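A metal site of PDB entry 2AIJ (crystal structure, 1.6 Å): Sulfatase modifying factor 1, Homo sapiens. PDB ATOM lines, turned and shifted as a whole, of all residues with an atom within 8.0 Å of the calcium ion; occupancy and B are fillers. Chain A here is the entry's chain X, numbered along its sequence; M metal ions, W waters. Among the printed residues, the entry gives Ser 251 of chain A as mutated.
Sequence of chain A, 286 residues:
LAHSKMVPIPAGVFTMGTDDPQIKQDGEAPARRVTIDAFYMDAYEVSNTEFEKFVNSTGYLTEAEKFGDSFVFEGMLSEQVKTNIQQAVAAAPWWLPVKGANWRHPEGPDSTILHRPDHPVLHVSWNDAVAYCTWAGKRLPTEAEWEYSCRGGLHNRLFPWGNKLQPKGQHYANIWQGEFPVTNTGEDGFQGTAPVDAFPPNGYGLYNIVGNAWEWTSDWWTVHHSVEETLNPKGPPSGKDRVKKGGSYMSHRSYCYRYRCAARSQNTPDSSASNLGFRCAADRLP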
ATOM      1  N   HIS A 171      37.902  31.782  14.590  1.00  0.00           N
ATOM      2  CA  HIS A 171      36.671  32.147  15.202  1.00  0.00           C
ATOM      3  C   HIS A 171      36.951  32.729  16.582  1.00  0.00           C
ATOM      4  O   HIS A 171      37.744  32.161  17.342  1.00  0.00           O
ATOM      5  CB  HIS A 171      35.736  30.932  15.323  1.00  0.00           C
ATOM      6  CG  HIS A 171      35.068  30.611  14.037  1.00  0.00           C
ATOM      7  ND1 HIS A 171      33.999  31.335  13.555  1.00  0.00           N
ATOM      8  CD2 HIS A 171      35.401  29.725  13.061  1.00  0.00           C
ATOM      9  CE1 HIS A 171      33.672  30.879  12.355  1.00  0.00           C
ATOM     10  NE2 HIS A 171      34.505  29.909  12.034  1.00  0.00           N
ATOM     11  N   ALA A 173      34.173  34.048  18.603  1.00  0.00           N
ATOM     12  CA  ALA A 173      32.938  34.014  19.374  1.00  0.00           C
ATOM     13  C   ALA A 173      32.029  32.904  18.861  1.00  0.00           C
ATOM     14  O   ALA A 173      32.153  32.479  17.693  1.00  0.00           O
ATOM     15  CB  ALA A 173      32.224  35.323  19.244  1.00  0.00           C
ATOM     16  N   ASN A 174      31.109  32.476  19.700  1.00  0.00           N
ATOM     17  CA  ASN A 174      30.185  31.428  19.343  1.00  0.00           C
ATOM     18  C   ASN A 174      28.884  32.067  18.868  1.00  0.00           C
ATOM     19  O   ASN A 174      28.067  32.486  19.643  1.00  0.00           O
ATOM     20  CB  ASN A 174      29.938  30.532  20.536  1.00  0.00           C
ATOM     21  CG  ASN A 174      28.954  29.449  20.236  1.00  0.00           C
ATOM     22  OD1 ASN A 174      28.723  29.158  19.068  1.00  0.00           O
ATOM     23  ND2 ASN A 174      28.322  28.892  21.270  1.00  0.00           N
ATOM     24  N   ILE A 175      28.709  32.108  17.554  1.00  0.00           N
ATOM     25  CA  ILE A 175      27.481  32.582  16.920  1.00  0.00           C
ATOM     26  C   ILE A 175      27.015  31.496  15.943  1.00  0.00           C
ATOM     27  O   ILE A 175      27.462  30.358  16.022  1.00  0.00           O
ATOM     28  CB  ILE A 175      27.674  33.961  16.269  1.00  0.00           C
ATOM     29  CG1 ILE A 175      28.771  33.983  15.205  1.00  0.00           C
ATOM     30  CG2 ILE A 175      27.998  34.977  17.371  1.00  0.00           C
ATOM     31  CD1 ILE A 175      28.808  35.243  14.360  1.00  0.00           C
ATOM     32  N   TRP A 176      26.159  31.838  14.995  1.00  0.00           N
ATOM     33  CA  TRP A 176      25.656  30.885  14.012  1.00  0.00           C
ATOM     34  C   TRP A 176      26.467  30.913  12.736  1.00  0.00           C
ATOM     35  O   TRP A 176      26.895  31.990  12.288  1.00  0.00           O
ATOM     36  CB  TRP A 176      24.220  31.272  13.687  1.00  0.00           C
ATOM     37  CG  TRP A 176      23.425  30.329  12.799  1.00  0.00           C
ATOM     38  CD1 TRP A 176      23.477  30.226  11.449  1.00  0.00           C
ATOM     39  CD2 TRP A 176      22.425  29.437  13.247  1.00  0.00           C
ATOM     40  NE1 TRP A 176      22.561  29.293  11.020  1.00  0.00           N
ATOM     41  CE2 TRP A 176      21.885  28.809  12.106  1.00  0.00           C
ATOM     42  CE3 TRP A 176      21.902  29.125  14.497  1.00  0.00           C
ATOM     43  CZ2 TRP A 176      20.858  27.841  12.192  1.00  0.00           C
ATOM     44  CZ3 TRP A 176      20.869  28.180  14.601  1.00  0.00           C
ATOM     45  CH2 TRP A 176      20.369  27.554  13.451  1.00  0.00           C
ATOM     46  N   GLN A 177      26.716  29.748  12.135  1.00  0.00           N
ATOM     47  CA  GLN A 177      27.191  29.718  10.761  1.00  0.00           C
ATOM     48  C   GLN A 177      26.226  28.888   9.984  1.00  0.00           C
ATOM     49  O   GLN A 177      25.802  27.871  10.467  1.00  0.00           O
ATOM     50  CB  GLN A 177      28.577  29.105  10.631  1.00  0.00           C
ATOM     51  CG  GLN A 177      29.686  29.938  11.252  1.00  0.00           C
ATOM     52  CD  GLN A 177      29.825  29.631  12.733  1.00  0.00           C
ATOM     53  OE1 GLN A 177      29.773  28.439  13.133  1.00  0.00           O
ATOM     54  NE2 GLN A 177      30.050  30.675  13.566  1.00  0.00           N
ATOM     55  N   ASN A 184      22.600  25.168  11.068  1.00  0.00           N
ATOM     56  CA  ASN A 184      23.781  25.637  11.787  1.00  0.00           C
ATOM     57  C   ASN A 184      24.891  24.628  11.554  1.00  0.00           C
ATOM     58  O   ASN A 184      24.804  23.480  12.001  1.00  0.00           O
ATOM     59  CB  ASN A 184      23.510  25.732  13.281  1.00  0.00           C
ATOM     60  CG  ASN A 184      24.620  26.434  14.027  1.00  0.00           C
ATOM     61  OD1 ASN A 184      25.731  26.589  13.517  1.00  0.00           O
ATOM     62  ND2 ASN A 184      24.293  26.887  15.253  1.00  0.00           N
ATOM     63  N   THR A 185      25.920  25.067  10.846  1.00  0.00           N
ATOM     64  CA  THR A 185      26.989  24.163  10.461  1.00  0.00           C
ATOM     65  C   THR A 185      27.906  23.806  11.617  1.00  0.00           C
ATOM     66  O   THR A 185      28.605  22.805  11.533  1.00  0.00           O
ATOM     67  CB  THR A 185      27.866  24.742   9.336  1.00  0.00           C
ATOM     68  OG1 THR A 185      28.572  25.869   9.870  1.00  0.00           O
ATOM     69  CG2 THR A 185      27.031  25.160   8.172  1.00  0.00           C
ATOM     70  N   GLY A 186      27.907  24.594  12.697  1.00  0.00           N
ATOM     71  CA  GLY A 186      28.824  24.320  13.813  1.00  0.00           C
ATOM     72  C   GLY A 186      30.287  24.504  13.473  1.00  0.00           C
ATOM     73  O   GLY A 186      31.167  23.968  14.133  1.00  0.00           O
ATOM     74  N   GLU A 187      30.547  25.300  12.436  1.00  0.00           N
ATOM     75  CA  GLU A 187      31.894  25.626  12.013  1.00  0.00           C
ATOM     76  C   GLU A 187      32.759  26.148  13.169  1.00  0.00           C
ATOM     77  O   GLU A 187      33.930  25.788  13.259  1.00  0.00           O
ATOM     78  CB  GLU A 187      31.807  26.658  10.906  1.00  0.00           C
ATOM     79  CG  GLU A 187      33.144  27.056  10.330  1.00  0.00           C
ATOM     80  CD  GLU A 187      33.053  28.243   9.382  1.00  0.00           C
ATOM     81  OE1 GLU A 187      32.026  28.442   8.723  1.00  0.00           O
ATOM     82  OE2 GLU A 187      34.055  28.994   9.361  1.00  0.00           O
ATOM     83  N   ASP A 188      32.178  26.970  14.069  1.00  0.00           N
ATOM     84  CA  ASP A 188      32.967  27.551  15.148  1.00  0.00           C
ATOM     85  C   ASP A 188      33.208  26.591  16.317  1.00  0.00           C
ATOM     86  O   ASP A 188      33.892  26.930  17.290  1.00  0.00           O
ATOM     87  CB  ASP A 188      32.374  28.869  15.624  1.00  0.00           C
ATOM     88  CG  ASP A 188      31.011  28.727  16.219  1.00  0.00           C
ATOM     89  OD1 ASP A 188      30.632  27.601  16.641  1.00  0.00           O
ATOM     90  OD2 ASP A 188      30.288  29.748  16.299  1.00  0.00           O
ATOM     91  N   GLY A 189      32.722  25.348  16.183  1.00  0.00           N
ATOM     92  CA  GLY A 189      32.961  24.333  17.210  1.00  0.00           C
ATOM     93  C   GLY A 189      31.799  24.040  18.136  1.00  0.00           C
ATOM     94  O   GLY A 189      31.862  23.100  18.912  1.00  0.00           O
ATOM     95  N   PHE A 190      30.729  24.847  18.045  1.00  0.00           N
ATOM     96  CA  PHE A 190      29.573  24.729  18.943  1.00  0.00           C
ATOM     97  C   PHE A 190      28.282  25.035  18.226  1.00  0.00           C
ATOM     98  O   PHE A 190      28.109  26.121  17.659  1.00  0.00           O
ATOM     99  CB  PHE A 190      29.770  25.687  20.120  1.00  0.00           C
ATOM    100  CG  PHE A 190      31.035  25.430  20.854  1.00  0.00           C
ATOM    101  CD1 PHE A 190      31.057  24.448  21.832  1.00  0.00           C
ATOM    102  CD2 PHE A 190      32.204  26.102  20.527  1.00  0.00           C
ATOM    103  CE1 PHE A 190      32.252  24.150  22.474  1.00  0.00           C
ATOM    104  CE2 PHE A 190      33.370  25.812  21.197  1.00  0.00           C
ATOM    105  CZ  PHE A 190      33.380  24.828  22.167  1.00  0.00           C
ATOM    106  N   GLN A 191      27.354  24.088  18.221  1.00  0.00           N
ATOM    107  CA  GLN A 191      26.009  24.380  17.721  1.00  0.00           C
ATOM    108  C   GLN A 191      25.157  25.166  18.731  1.00  0.00           C
ATOM    109  O   GLN A 191      24.562  26.197  18.416  1.00  0.00           O
ATOM    110  CB  GLN A 191      25.340  23.101  17.300  1.00  0.00           C
ATOM    111  CG  GLN A 191      25.919  22.705  15.974  1.00  0.00           C
ATOM    112  CD  GLN A 191      25.516  21.373  15.480  1.00  0.00           C
ATOM    113  OE1 GLN A 191      25.501  20.391  16.242  1.00  0.00           O
ATOM    114  NE2 GLN A 191      25.267  21.296  14.171  1.00  0.00           N
ATOM    115  N   GLY A 192      25.086  24.647  19.963  1.00  0.00           N
ATOM    116  CA  GLY A 192      24.470  25.381  21.036  1.00  0.00           C
ATOM    117  C   GLY A 192      25.498  26.206  21.782  1.00  0.00           C
ATOM    118  O   GLY A 192      26.401  26.772  21.166  1.00  0.00           O
ATOM    119  N   THR A 193      25.391  26.254  23.110  1.00  0.00           N
ATOM    120  CA  THR A 193      26.380  26.957  23.873  1.00  0.00           C
ATOM    121  C   THR A 193      27.740  26.281  23.873  1.00  0.00           C
ATOM    122  O   THR A 193      27.883  25.093  23.504  1.00  0.00           O
ATOM    123  CB  THR A 193      25.899  27.143  25.345  1.00  0.00           C
ATOM    124  OG1 THR A 193      25.598  25.872  25.920  1.00  0.00           O
ATOM    125  CG2 THR A 193      24.657  27.990  25.355  1.00  0.00           C
ATOM    126  N   ALA A 194      28.712  27.063  24.322  1.00  0.00           N
ATOM    127  CA  ALA A 194      30.095  26.636  24.554  1.00  0.00           C
ATOM    128  C   ALA A 194      30.395  26.843  26.022  1.00  0.00           C
ATOM    129  O   ALA A 194      29.741  27.653  26.671  1.00  0.00           O
ATOM    130  CB  ALA A 194      31.077  27.497  23.749  1.00  0.00           C
ATOM    131  N   PHE A 199      36.848  30.330  23.607  1.00  0.00           N
ATOM    132  CA  PHE A 199      37.261  31.437  22.681  1.00  0.00           C
ATOM    133  C   PHE A 199      38.213  32.399  23.349  1.00  0.00           C
ATOM    134  O   PHE A 199      38.427  32.306  24.535  1.00  0.00           O
ATOM    135  CB  PHE A 199      36.038  32.126  22.077  1.00  0.00           C
ATOM    136  CG  PHE A 199      35.249  31.191  21.192  1.00  0.00           C
ATOM    137  CD1 PHE A 199      35.716  30.895  19.943  1.00  0.00           C
ATOM    138  CD2 PHE A 199      34.130  30.548  21.647  1.00  0.00           C
ATOM    139  CE1 PHE A 199      35.044  29.982  19.147  1.00  0.00           C
ATOM    140  CE2 PHE A 199      33.476  29.628  20.838  1.00  0.00           C
ATOM    141  CZ  PHE A 199      33.917  29.365  19.583  1.00  0.00           C
ATOM    142  N   ASN A 212      27.507  33.310  22.411  1.00  0.00           N
ATOM    143  CA  ASN A 212      27.236  32.298  23.426  1.00  0.00           C
ATOM    144  C   ASN A 212      25.867  32.539  24.014  1.00  0.00           C
ATOM    145  O   ASN A 212      24.893  32.153  23.367  1.00  0.00           O
ATOM    146  CB  ASN A 212      28.384  32.180  24.460  1.00  0.00           C
ATOM    147  CG  ASN A 212      28.642  30.738  24.871  1.00  0.00           C
ATOM    148  OD1 ASN A 212      28.445  29.811  24.052  1.00  0.00           O
ATOM    149  ND2 ASN A 212      29.132  30.510  26.100  1.00  0.00           N
ATOM    150  N   SER A 248      24.175  35.925  20.830  1.00  0.00           N
ATOM    151  CA  SER A 248      24.190  34.553  21.329  1.00  0.00           C
ATOM    152  C   SER A 248      24.690  33.611  20.238  1.00  0.00           C
ATOM    153  O   SER A 248      24.963  34.001  19.096  1.00  0.00           O
ATOM    154  CB  SER A 248      22.790  34.132  21.758  1.00  0.00           C
ATOM    155  OG  SER A 248      21.957  33.793  20.639  1.00  0.00           O
ATOM    156  N   TYR A 249      24.687  32.325  20.591  1.00  0.00           N
ATOM    157  CA  TYR A 249      25.025  31.276  19.625  1.00  0.00           C
ATOM    158  C   TYR A 249      24.098  31.172  18.411  1.00  0.00           C
ATOM    159  O   TYR A 249      24.439  30.518  17.394  1.00  0.00           O
ATOM    160  CB  TYR A 249      25.098  29.935  20.354  1.00  0.00           C
ATOM    161  CG  TYR A 249      23.797  29.368  20.841  1.00  0.00           C
ATOM    162  CD1 TYR A 249      23.381  29.464  22.203  1.00  0.00           C
ATOM    163  CD2 TYR A 249      23.007  28.647  19.970  1.00  0.00           C
ATOM    164  CE1 TYR A 249      22.176  28.883  22.623  1.00  0.00           C
ATOM    165  CE2 TYR A 249      21.805  28.094  20.379  1.00  0.00           C
ATOM    166  CZ  TYR A 249      21.411  28.195  21.695  1.00  0.00           C
ATOM    167  OH  TYR A 249      20.229  27.591  22.071  1.00  0.00           O
ATOM    168  N   MET A 250      22.961  31.848  18.498  1.00  0.00           N
ATOM    169  CA  MET A 250      21.960  31.913  17.406  1.00  0.00           C
ATOM    170  C   MET A 250      22.189  33.078  16.466  1.00  0.00           C
ATOM    171  O   MET A 250      21.581  33.155  15.393  1.00  0.00           O
ATOM    172  CB  MET A 250      20.548  32.002  17.996  1.00  0.00           C
ATOM    173  CG  MET A 250      20.029  30.737  18.644  1.00  0.00           C
ATOM    174  SD  MET A 250      18.471  31.024  19.500  1.00  0.00           S
ATOM    175  CE  MET A 250      17.329  31.228  18.131  1.00  0.00           C
ATOM    176  N   SER A 251      23.008  34.058  16.853  1.00  0.00           N
ATOM    177  CA  SER A 251      23.075  35.280  16.114  1.00  0.00           C
ATOM    178  C   SER A 251      23.757  35.081  14.763  1.00  0.00           C
ATOM    179  O   SER A 251      24.701  34.312  14.638  1.00  0.00           O
ATOM    180  CB  SER A 251      23.805  36.360  16.906  1.00  0.00           C
ATOM    181  OG  SER A 251      23.157  36.602  18.157  1.00  0.00           O
HETATM  182 CA    CA M   1      28.307  28.381  16.997  1.00  0.00          CA
HETATM  183  O   HOH W   1      25.944  28.307  17.293  1.00  0.00           O
HETATM  184  O   HOH W   2      27.977  27.412  14.775  1.00  0.00           O
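ND2 of Asn 174 is in hydrogen-bond range of O of Gly 192, at 2.9 Å. The backbone NH (N) of Asp 188 is in hydrogen-bond range of the side-chain amide oxygen (OE1) of Gln 177 (3.0 Å). The side-chain amide oxygen (OD1) of Asn 212 is in hydrogen-bond range of the side-chain amide nitrogen (ND2) of Asn 174.
Within 4 Å of the calcium ion: Asn 174, Ile 175, Asp 188 and Phe 190.
The calcium ion is bound by the side-chain amide oxygen (OD1) of Asn 174 (2.3 Å), the backbone carbonyl oxygen (O) of Ile 175 (2.4 Å), the backbone carbonyl oxygen (O) of Phe 190 (2.4 Å), water W1 (2.4 Å), water W2 (2.4 Å), the side-chain carboxylate (OD1) of Asp 188 (2.5 Å) and the side-chain carboxylate (OD2) of Asp 188 (2.5 Å). The calcium ion has seven donor atoms within binding distance.
Water W1 lies within hydrogen-bond range of the backbone carbonyl oxygen of Tyr 249 (2.7 Å), the backbone carbonyl oxygen of Gln 191 (2.8 Å) and the side-chain amide nitrogen of Asn 184 (3.0 Å). Water W2 bridges the side-chain amide oxygen (OE1) of Gln 177 (2.6 Å) and the side-chain amide oxygen (OD1) of Asn 184 (2.7 Å).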
